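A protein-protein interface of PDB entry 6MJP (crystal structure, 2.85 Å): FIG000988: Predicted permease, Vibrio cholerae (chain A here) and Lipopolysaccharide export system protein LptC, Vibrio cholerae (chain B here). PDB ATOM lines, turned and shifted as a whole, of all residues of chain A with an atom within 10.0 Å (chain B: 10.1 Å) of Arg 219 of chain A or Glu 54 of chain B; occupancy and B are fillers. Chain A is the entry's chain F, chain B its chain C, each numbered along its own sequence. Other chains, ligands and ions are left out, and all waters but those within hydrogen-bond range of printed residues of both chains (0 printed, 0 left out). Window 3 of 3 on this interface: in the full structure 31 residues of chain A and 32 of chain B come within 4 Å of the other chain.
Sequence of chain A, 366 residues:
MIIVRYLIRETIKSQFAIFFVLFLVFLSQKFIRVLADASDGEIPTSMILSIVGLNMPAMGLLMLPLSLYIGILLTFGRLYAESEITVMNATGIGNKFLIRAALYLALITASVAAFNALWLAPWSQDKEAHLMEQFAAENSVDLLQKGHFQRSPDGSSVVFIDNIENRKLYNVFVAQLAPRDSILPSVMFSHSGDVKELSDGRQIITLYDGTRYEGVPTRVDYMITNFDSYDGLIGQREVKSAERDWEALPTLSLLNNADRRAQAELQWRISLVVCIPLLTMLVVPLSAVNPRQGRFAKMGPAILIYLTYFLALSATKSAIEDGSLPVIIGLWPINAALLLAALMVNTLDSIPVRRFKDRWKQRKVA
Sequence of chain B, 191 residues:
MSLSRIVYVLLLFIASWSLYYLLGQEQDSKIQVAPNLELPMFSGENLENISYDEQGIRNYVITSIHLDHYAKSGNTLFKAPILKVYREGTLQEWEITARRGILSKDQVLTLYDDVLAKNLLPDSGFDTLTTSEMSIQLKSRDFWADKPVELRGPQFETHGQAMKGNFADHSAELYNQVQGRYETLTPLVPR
The backbone carbonyl oxygen of Tyr 222 of chain A is in hydrogen-bond range of the backbone NH of Tyr 52 of chain B (3.2 Å).
NH2 of Arg 219 of chain A is in salt-bridge range of OE2 of Glu 54 of chain B (3.5 Å).
The backbone carbonyl oxygen of Ser 51 of chain B sits at hydrogen-bond distance from the backbone NH of Asn 59 of chain B.
N of Ser 51 of chain B sits at hydrogen-bond distance from O of Tyr 60 of chain B, at 3.0 Å.
The side-chain hydroxyl (OH) of Tyr 222 of chain A sits at hydrogen-bond distance from the backbone carbonyl oxygen (O) of Val 216 of chain A, 3.2 Å away.
The side-chain carboxylate (OD2) of Asp 221 of chain A is in salt-bridge range of the guanidinium group (NH1) of Arg 219 of chain A (3.5 Å).
Among the printed residues, pairs that only touch across the chains: Val 220 of chain A with Gly 56 of chain B, Asp 221 of chain A with Tyr 52 of chain B, Asp 221 of chain A with Asp 53 of chain B, Tyr 222 of chain A with Ser 51 of chain B and Ile 224 of chain A with Tyr 52 of chain B.
No residue of chain B comes within 4 Å of Thr 218 of chain A.
Of chain B, only Glu 54 comes within 4 Å of Arg 219 of chain A.
Of chain B, only Gly 56 (3.9 Å) comes within 4 Å of Val 220 of chain A.
Asp 221 of chain A touches two residues of chain B.
Printed residues of chain B within 4 Å of Tyr 222 of chain A: Ser 51 (3.9 Å) and Tyr 52 (3.2 Å).
Of the printed residues of chain B, Ile 224 of chain A touches Tyr 52 (3.8 Å).
Of the printed residues of chain A, Ser 51 of chain B touches Tyr 222 (3.9 Å).
Of the printed residues of chain A, Tyr 52 of chain B touches Asp 221, Tyr 222 and Ile 224.
Asp 53 of chain B touches one residue of chain A.
Printed residues of chain A within 4 Å of Gly 56 of chain B: Val 220 (3.9 Å).
Arg 58 of chain B touches none of the printed residues of chain A.
Of the 13 printed residues of chain A, 5 touch a printed residue of chain B.
Among the printed residues, Asp or Glu carboxylates within 4 Å of a Lys or Arg side-chain nitrogen of the other chain: Arg 219 of chain A with Glu 54 of chain B (3.5 Å).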
ATOM      1  N   LEU A 184      17.204 -26.272   9.034  1.00  0.00           N
ATOM      2  CA  LEU A 184      17.752 -25.237   9.893  1.00  0.00           C
ATOM      3  C   LEU A 184      18.647 -25.848  10.961  1.00  0.00           C
ATOM      4  O   LEU A 184      18.515 -27.030  11.296  1.00  0.00           O
ATOM      5  CB  LEU A 184      16.614 -24.446  10.541  1.00  0.00           C
ATOM      6  CG  LEU A 184      15.606 -23.860   9.556  1.00  0.00           C
ATOM      7  CD1 LEU A 184      14.480 -23.158  10.294  1.00  0.00           C
ATOM      8  CD2 LEU A 184      16.308 -22.905   8.613  1.00  0.00           C
ATOM      9  N   PRO A 185      19.577 -25.064  11.519  1.00  0.00           N
ATOM     10  CA  PRO A 185      20.404 -25.575  12.619  1.00  0.00           C
ATOM     11  C   PRO A 185      19.552 -26.017  13.798  1.00  0.00           C
ATOM     12  O   PRO A 185      18.442 -25.528  14.018  1.00  0.00           O
ATOM     13  CB  PRO A 185      21.288 -24.379  12.991  1.00  0.00           C
ATOM     14  CG  PRO A 185      20.578 -23.182  12.424  1.00  0.00           C
ATOM     15  CD  PRO A 185      19.923 -23.676  11.174  1.00  0.00           C
ATOM     16  N   GLU A 214      15.093 -26.676  17.283  1.00  0.00           N
ATOM     17  CA  GLU A 214      15.516 -26.128  15.994  1.00  0.00           C
ATOM     18  C   GLU A 214      15.464 -24.605  16.050  1.00  0.00           C
ATOM     19  O   GLU A 214      14.382 -24.018  16.154  1.00  0.00           O
ATOM     20  CB  GLU A 214      14.635 -26.649  14.859  1.00  0.00           C
ATOM     21  CG  GLU A 214      15.163 -26.306  13.472  1.00  0.00           C
ATOM     22  CD  GLU A 214      14.341 -26.912  12.350  1.00  0.00           C
ATOM     23  OE1 GLU A 214      13.099 -26.856  12.426  1.00  0.00           O
ATOM     24  OE2 GLU A 214      14.941 -27.451  11.393  1.00  0.00           O
ATOM     25  N   GLY A 215      16.622 -23.962  15.960  1.00  0.00           N
ATOM     26  CA  GLY A 215      16.653 -22.518  16.037  1.00  0.00           C
ATOM     27  C   GLY A 215      18.071 -22.000  16.166  1.00  0.00           C
ATOM     28  O   GLY A 215      19.040 -22.732  15.974  1.00  0.00           O
ATOM     29  N   VAL A 216      18.163 -20.714  16.492  1.00  0.00           N
ATOM     30  CA  VAL A 216      19.436 -20.006  16.609  1.00  0.00           C
ATOM     31  C   VAL A 216      19.454 -19.262  17.942  1.00  0.00           C
ATOM     32  O   VAL A 216      18.410 -18.741  18.370  1.00  0.00           O
ATOM     33  CB  VAL A 216      19.646 -19.060  15.414  1.00  0.00           C
ATOM     34  CG1 VAL A 216      20.841 -18.146  15.630  1.00  0.00           C
ATOM     35  CG2 VAL A 216      19.832 -19.862  14.136  1.00  0.00           C
ATOM     36  N   PRO A 217      20.597 -19.209  18.639  1.00  0.00           N
ATOM     37  CA  PRO A 217      20.639 -18.517  19.943  1.00  0.00           C
ATOM     38  C   PRO A 217      20.186 -17.064  19.908  1.00  0.00           C
ATOM     39  O   PRO A 217      19.677 -16.564  20.924  1.00  0.00           O
ATOM     40  CB  PRO A 217      22.117 -18.633  20.340  1.00  0.00           C
ATOM     41  CG  PRO A 217      22.569 -19.888  19.687  1.00  0.00           C
ATOM     42  CD  PRO A 217      21.831 -19.973  18.382  1.00  0.00           C
ATOM     43  N   THR A 218      20.368 -16.367  18.785  1.00  0.00           N
ATOM     44  CA  THR A 218      19.983 -14.965  18.676  1.00  0.00           C
ATOM     45  C   THR A 218      18.498 -14.781  18.361  1.00  0.00           C
ATOM     46  O   THR A 218      17.864 -13.867  18.900  1.00  0.00           O
ATOM     47  CB  THR A 218      20.847 -14.276  17.618  1.00  0.00           C
ATOM     48  OG1 THR A 218      20.835 -15.046  16.413  1.00  0.00           O
ATOM     49  CG2 THR A 218      22.277 -14.163  18.105  1.00  0.00           C
ATOM     50  N   ARG A 219      17.918 -15.626  17.508  1.00  0.00           N
ATOM     51  CA  ARG A 219      16.492 -15.542  17.223  1.00  0.00           C
ATOM     52  C   ARG A 219      15.679 -16.313  18.268  1.00  0.00           C
ATOM     53  O   ARG A 219      16.220 -17.038  19.108  1.00  0.00           O
ATOM     54  CB  ARG A 219      16.187 -16.070  15.820  1.00  0.00           C
ATOM     55  CG  ARG A 219      16.040 -14.990  14.757  1.00  0.00           C
ATOM     56  CD  ARG A 219      15.440 -15.557  13.478  1.00  0.00           C
ATOM     57  NE  ARG A 219      14.873 -14.514  12.631  1.00  0.00           N
ATOM     58  CZ  ARG A 219      14.180 -14.747  11.519  1.00  0.00           C
ATOM     59  NH1 ARG A 219      13.968 -15.993  11.117  1.00  0.00           N
ATOM     60  NH2 ARG A 219      13.698 -13.735  10.810  1.00  0.00           N
ATOM     61  N   VAL A 220      14.356 -16.160  18.196  1.00  0.00           N
ATOM     62  CA  VAL A 220      13.456 -16.734  19.192  1.00  0.00           C
ATOM     63  C   VAL A 220      12.440 -17.715  18.605  1.00  0.00           C
ATOM     64  O   VAL A 220      11.909 -18.552  19.351  1.00  0.00           O
ATOM     65  CB  VAL A 220      12.723 -15.626  19.979  1.00  0.00           C
ATOM     66  CG1 VAL A 220      12.110 -16.183  21.249  1.00  0.00           C
ATOM     67  CG2 VAL A 220      13.670 -14.491  20.318  1.00  0.00           C
ATOM     68  N   ASP A 221      12.134 -17.660  17.311  1.00  0.00           N
ATOM     69  CA  ASP A 221      11.229 -18.629  16.694  1.00  0.00           C
ATOM     70  C   ASP A 221      11.903 -19.994  16.646  1.00  0.00           C
ATOM     71  O   ASP A 221      12.765 -20.239  15.800  1.00  0.00           O
ATOM     72  CB  ASP A 221      10.830 -18.165  15.298  1.00  0.00           C
ATOM     73  CG  ASP A 221      12.008 -17.649  14.486  1.00  0.00           C
ATOM     74  OD1 ASP A 221      12.874 -16.956  15.062  1.00  0.00           O
ATOM     75  OD2 ASP A 221      12.066 -17.938  13.272  1.00  0.00           O
ATOM     76  N   TYR A 222      11.528 -20.892  17.556  1.00  0.00           N
ATOM     77  CA  TYR A 222      12.073 -22.244  17.582  1.00  0.00           C
ATOM     78  C   TYR A 222      11.046 -23.237  17.046  1.00  0.00           C
ATOM     79  O   TYR A 222       9.896 -22.895  16.766  1.00  0.00           O
ATOM     80  CB  TYR A 222      12.502 -22.658  19.001  1.00  0.00           C
ATOM     81  CG  TYR A 222      13.782 -22.013  19.519  1.00  0.00           C
ATOM     82  CD1 TYR A 222      15.034 -22.501  19.160  1.00  0.00           C
ATOM     83  CD2 TYR A 222      13.730 -20.932  20.390  1.00  0.00           C
ATOM     84  CE1 TYR A 222      16.199 -21.910  19.640  1.00  0.00           C
ATOM     85  CE2 TYR A 222      14.884 -20.343  20.872  1.00  0.00           C
ATOM     86  CZ  TYR A 222      16.112 -20.829  20.499  1.00  0.00           C
ATOM     87  OH  TYR A 222      17.246 -20.217  20.994  1.00  0.00           O
ATOM     88  N   MET A 223      11.485 -24.483  16.890  1.00  0.00           N
ATOM     89  CA  MET A 223      10.582 -25.613  16.719  1.00  0.00           C
ATOM     90  C   MET A 223      11.069 -26.728  17.631  1.00  0.00           C
ATOM     91  O   MET A 223      12.191 -27.215  17.476  1.00  0.00           O
ATOM     92  CB  MET A 223      10.509 -26.089  15.267  1.00  0.00           C
ATOM     93  CG  MET A 223       9.302 -26.979  15.008  1.00  0.00           C
ATOM     94  SD  MET A 223       9.566 -28.215  13.725  1.00  0.00           S
ATOM     95  CE  MET A 223       9.881 -27.175  12.302  1.00  0.00           C
ATOM     96  N   ILE A 224      10.231 -27.118  18.583  1.00  0.00           N
ATOM     97  CA  ILE A 224      10.575 -28.110  19.589  1.00  0.00           C
ATOM     98  C   ILE A 224       9.889 -29.410  19.209  1.00  0.00           C
ATOM     99  O   ILE A 224       8.669 -29.441  19.015  1.00  0.00           O
ATOM    100  CB  ILE A 224      10.157 -27.654  20.994  1.00  0.00           C
ATOM    101  CG1 ILE A 224      10.453 -26.167  21.186  1.00  0.00           C
ATOM    102  CG2 ILE A 224      10.878 -28.469  22.047  1.00  0.00           C
ATOM    103  CD1 ILE A 224      11.908 -25.813  21.018  1.00  0.00           C
ATOM    104  N   SER B  51       5.651 -25.233  16.998  1.00  0.00           N
ATOM    105  CA  SER B  51       6.272 -24.162  16.230  1.00  0.00           C
ATOM    106  C   SER B  51       5.865 -22.796  16.763  1.00  0.00           C
ATOM    107  O   SER B  51       4.697 -22.568  17.083  1.00  0.00           O
ATOM    108  CB  SER B  51       5.902 -24.264  14.767  1.00  0.00           C
ATOM    109  OG  SER B  51       6.059 -23.019  14.117  1.00  0.00           O
ATOM    110  N   TYR B  52       6.828 -21.879  16.825  1.00  0.00           N
ATOM    111  CA  TYR B  52       6.625 -20.578  17.447  1.00  0.00           C
ATOM    112  C   TYR B  52       6.748 -19.462  16.414  1.00  0.00           C
ATOM    113  O   TYR B  52       7.290 -19.654  15.321  1.00  0.00           O
ATOM    114  CB  TYR B  52       7.626 -20.362  18.589  1.00  0.00           C
ATOM    115  CG  TYR B  52       7.481 -21.349  19.734  1.00  0.00           C
ATOM    116  CD1 TYR B  52       7.831 -22.687  19.579  1.00  0.00           C
ATOM    117  CD2 TYR B  52       7.006 -20.938  20.970  1.00  0.00           C
ATOM    118  CE1 TYR B  52       7.701 -23.582  20.619  1.00  0.00           C
ATOM    119  CE2 TYR B  52       6.874 -21.824  22.013  1.00  0.00           C
ATOM    120  CZ  TYR B  52       7.221 -23.142  21.835  1.00  0.00           C
ATOM    121  OH  TYR B  52       7.081 -24.012  22.888  1.00  0.00           O
ATOM    122  N   ASP B  53       6.217 -18.289  16.765  1.00  0.00           N
ATOM    123  CA  ASP B  53       6.270 -17.125  15.895  1.00  0.00           C
ATOM    124  C   ASP B  53       7.546 -16.333  16.164  1.00  0.00           C
ATOM    125  O   ASP B  53       8.302 -16.628  17.090  1.00  0.00           O
ATOM    126  CB  ASP B  53       5.028 -16.251  16.088  1.00  0.00           C
ATOM    127  N   GLU B  54       7.783 -15.298  15.351  1.00  0.00           N
ATOM    128  CA  GLU B  54       9.017 -14.523  15.449  1.00  0.00           C
ATOM    129  C   GLU B  54       9.107 -13.708  16.735  1.00  0.00           C
ATOM    130  O   GLU B  54      10.160 -13.119  17.005  1.00  0.00           O
ATOM    131  CB  GLU B  54       9.162 -13.601  14.233  1.00  0.00           C
ATOM    132  CG  GLU B  54      10.581 -13.082  14.009  1.00  0.00           C
ATOM    133  CD  GLU B  54      10.791 -12.507  12.624  1.00  0.00           C
ATOM    134  OE1 GLU B  54      10.215 -13.057  11.662  1.00  0.00           O
ATOM    135  OE2 GLU B  54      11.533 -11.508  12.498  1.00  0.00           O
ATOM    136  N   GLN B  55       8.050 -13.665  17.538  1.00  0.00           N
ATOM    137  CA  GLN B  55       8.097 -12.975  18.816  1.00  0.00           C
ATOM    138  C   GLN B  55       8.156 -13.924  20.007  1.00  0.00           C
ATOM    139  O   GLN B  55       8.276 -13.455  21.144  1.00  0.00           O
ATOM    140  CB  GLN B  55       6.879 -12.044  18.952  1.00  0.00           C
ATOM    141  CG  GLN B  55       6.854 -10.938  17.910  1.00  0.00           C
ATOM    142  CD  GLN B  55       5.579 -10.127  17.953  1.00  0.00           C
ATOM    143  OE1 GLN B  55       4.608 -10.506  18.611  1.00  0.00           O
ATOM    144  NE2 GLN B  55       5.571  -8.999  17.250  1.00  0.00           N
ATOM    145  N   GLY B  56       8.087 -15.230  19.782  1.00  0.00           N
ATOM    146  CA  GLY B  56       8.220 -16.198  20.850  1.00  0.00           C
ATOM    147  C   GLY B  56       6.934 -16.795  21.374  1.00  0.00           C
ATOM    148  O   GLY B  56       6.942 -17.359  22.474  1.00  0.00           O
ATOM    149  N   ILE B  57       5.838 -16.700  20.632  1.00  0.00           N
ATOM    150  CA  ILE B  57       4.543 -17.202  21.078  1.00  0.00           C
ATOM    151  C   ILE B  57       4.247 -18.499  20.339  1.00  0.00           C
ATOM    152  O   ILE B  57       4.524 -18.619  19.139  1.00  0.00           O
ATOM    153  CB  ILE B  57       3.435 -16.153  20.844  1.00  0.00           C
ATOM    154  CG1 ILE B  57       3.825 -14.805  21.462  1.00  0.00           C
ATOM    155  CG2 ILE B  57       2.099 -16.626  21.408  1.00  0.00           C
ATOM    156  CD1 ILE B  57       4.040 -14.848  22.958  1.00  0.00           C
ATOM    157  N   ARG B  58       3.696 -19.477  21.054  1.00  0.00           N
ATOM    158  CA  ARG B  58       3.336 -20.754  20.447  1.00  0.00           C
ATOM    159  C   ARG B  58       2.370 -20.571  19.273  1.00  0.00           C
ATOM    160  O   ARG B  58       1.198 -20.252  19.480  1.00  0.00           O
ATOM    161  CB  ARG B  58       2.729 -21.675  21.513  1.00  0.00           C
ATOM    162  CG  ARG B  58       2.352 -23.062  21.007  1.00  0.00           C
ATOM    163  CD  ARG B  58       2.039 -24.023  22.149  1.00  0.00           C
ATOM    164  NE  ARG B  58       0.884 -23.606  22.938  1.00  0.00           N
ATOM    165  CZ  ARG B  58       0.321 -24.339  23.894  1.00  0.00           C
ATOM    166  NH1 ARG B  58      -0.727 -23.873  24.555  1.00  0.00           N
ATOM    167  NH2 ARG B  58       0.802 -25.538  24.187  1.00  0.00           N
ATOM    168  N   ASN B  59       2.848 -20.773  18.040  1.00  0.00           N
ATOM    169  CA  ASN B  59       2.005 -20.599  16.858  1.00  0.00           C
ATOM    170  C   ASN B  59       1.066 -21.793  16.656  1.00  0.00           C
ATOM    171  O   ASN B  59      -0.152 -21.624  16.539  1.00  0.00           O
ATOM    172  CB  ASN B  59       2.888 -20.369  15.618  1.00  0.00           C
ATOM    173  CG  ASN B  59       2.092 -19.934  14.378  1.00  0.00           C
ATOM    174  OD1 ASN B  59       1.040 -19.299  14.474  1.00  0.00           O
ATOM    175  ND2 ASN B  59       2.615 -20.265  13.202  1.00  0.00           N
ATOM    176  N   TYR B  60       1.610 -23.008  16.616  1.00  0.00           N
ATOM    177  CA  TYR B  60       0.801 -24.196  16.362  1.00  0.00           C
ATOM    178  C   TYR B  60       1.546 -25.417  16.886  1.00  0.00           C
ATOM    179  O   TYR B  60       2.708 -25.335  17.290  1.00  0.00           O
ATOM    180  CB  TYR B  60       0.472 -24.353  14.866  1.00  0.00           C
ATOM    181  CG  TYR B  60       1.693 -24.557  14.001  1.00  0.00           C
ATOM    182  CD1 TYR B  60       2.235 -25.824  13.812  1.00  0.00           C
ATOM    183  CD2 TYR B  60       2.318 -23.483  13.386  1.00  0.00           C
ATOM    184  CE1 TYR B  60       3.366 -26.016  13.038  1.00  0.00           C
ATOM    185  CE2 TYR B  60       3.445 -23.665  12.601  1.00  0.00           C
ATOM    186  CZ  TYR B  60       3.958 -24.938  12.426  1.00  0.00           C
ATOM    187  OH  TYR B  60       5.082 -25.140  11.661  1.00  0.00           O
ATOM    188  N   GLN B 107       6.386 -23.191   4.763  1.00  0.00           N
ATOM    189  CA  GLN B 107       5.434 -23.328   5.871  1.00  0.00           C
ATOM    190  C   GLN B 107       4.006 -23.525   5.368  1.00  0.00           C
ATOM    191  O   GLN B 107       3.082 -22.846   5.820  1.00  0.00           O
ATOM    192  CB  GLN B 107       5.507 -22.093   6.794  1.00  0.00           C
ATOM    193  CG  GLN B 107       4.906 -22.225   8.192  1.00  0.00           C
ATOM    194  CD  GLN B 107       5.784 -22.993   9.189  1.00  0.00           C
ATOM    195  OE1 GLN B 107       5.364 -23.277  10.314  1.00  0.00           O
ATOM    196  NE2 GLN B 107       6.994 -23.345   8.772  1.00  0.00           N
ATOM    197  N   LYS B 139       1.529 -19.644   8.883  1.00  0.00           N
ATOM    198  CA  LYS B 139       1.854 -18.245   9.141  1.00  0.00           C
ATOM    199  C   LYS B 139       0.632 -17.352   8.944  1.00  0.00           C
ATOM    200  O   LYS B 139       0.156 -16.712   9.889  1.00  0.00           O
ATOM    201  CB  LYS B 139       3.010 -17.802   8.245  1.00  0.00           C
ATOM    202  CG  LYS B 139       2.993 -18.423   6.858  1.00  0.00           C
ATOM    203  N   ARG B 141      -2.354 -18.411   8.169  1.00  0.00           N
ATOM    204  CA  ARG B 141      -3.524 -19.226   8.490  1.00  0.00           C
ATOM    205  C   ARG B 141      -4.525 -19.322   7.339  1.00  0.00           C
ATOM    206  O   ARG B 141      -5.610 -19.892   7.511  1.00  0.00           O
ATOM    207  CB  ARG B 141      -4.216 -18.730   9.766  1.00  0.00           C
ATOM    208  CG  ARG B 141      -3.576 -19.303  11.015  1.00  0.00           C
ATOM    209  CD  ARG B 141      -3.633 -18.344  12.185  1.00  0.00           C
ATOM    210  NE  ARG B 141      -2.993 -18.919  13.364  1.00  0.00           N
ATOM    211  CZ  ARG B 141      -1.679 -19.055  13.511  1.00  0.00           C
ATOM    212  NH1 ARG B 141      -0.856 -18.666  12.547  1.00  0.00           N
ATOM    213  NH2 ARG B 141      -1.185 -19.584  14.624  1.00  0.00           N
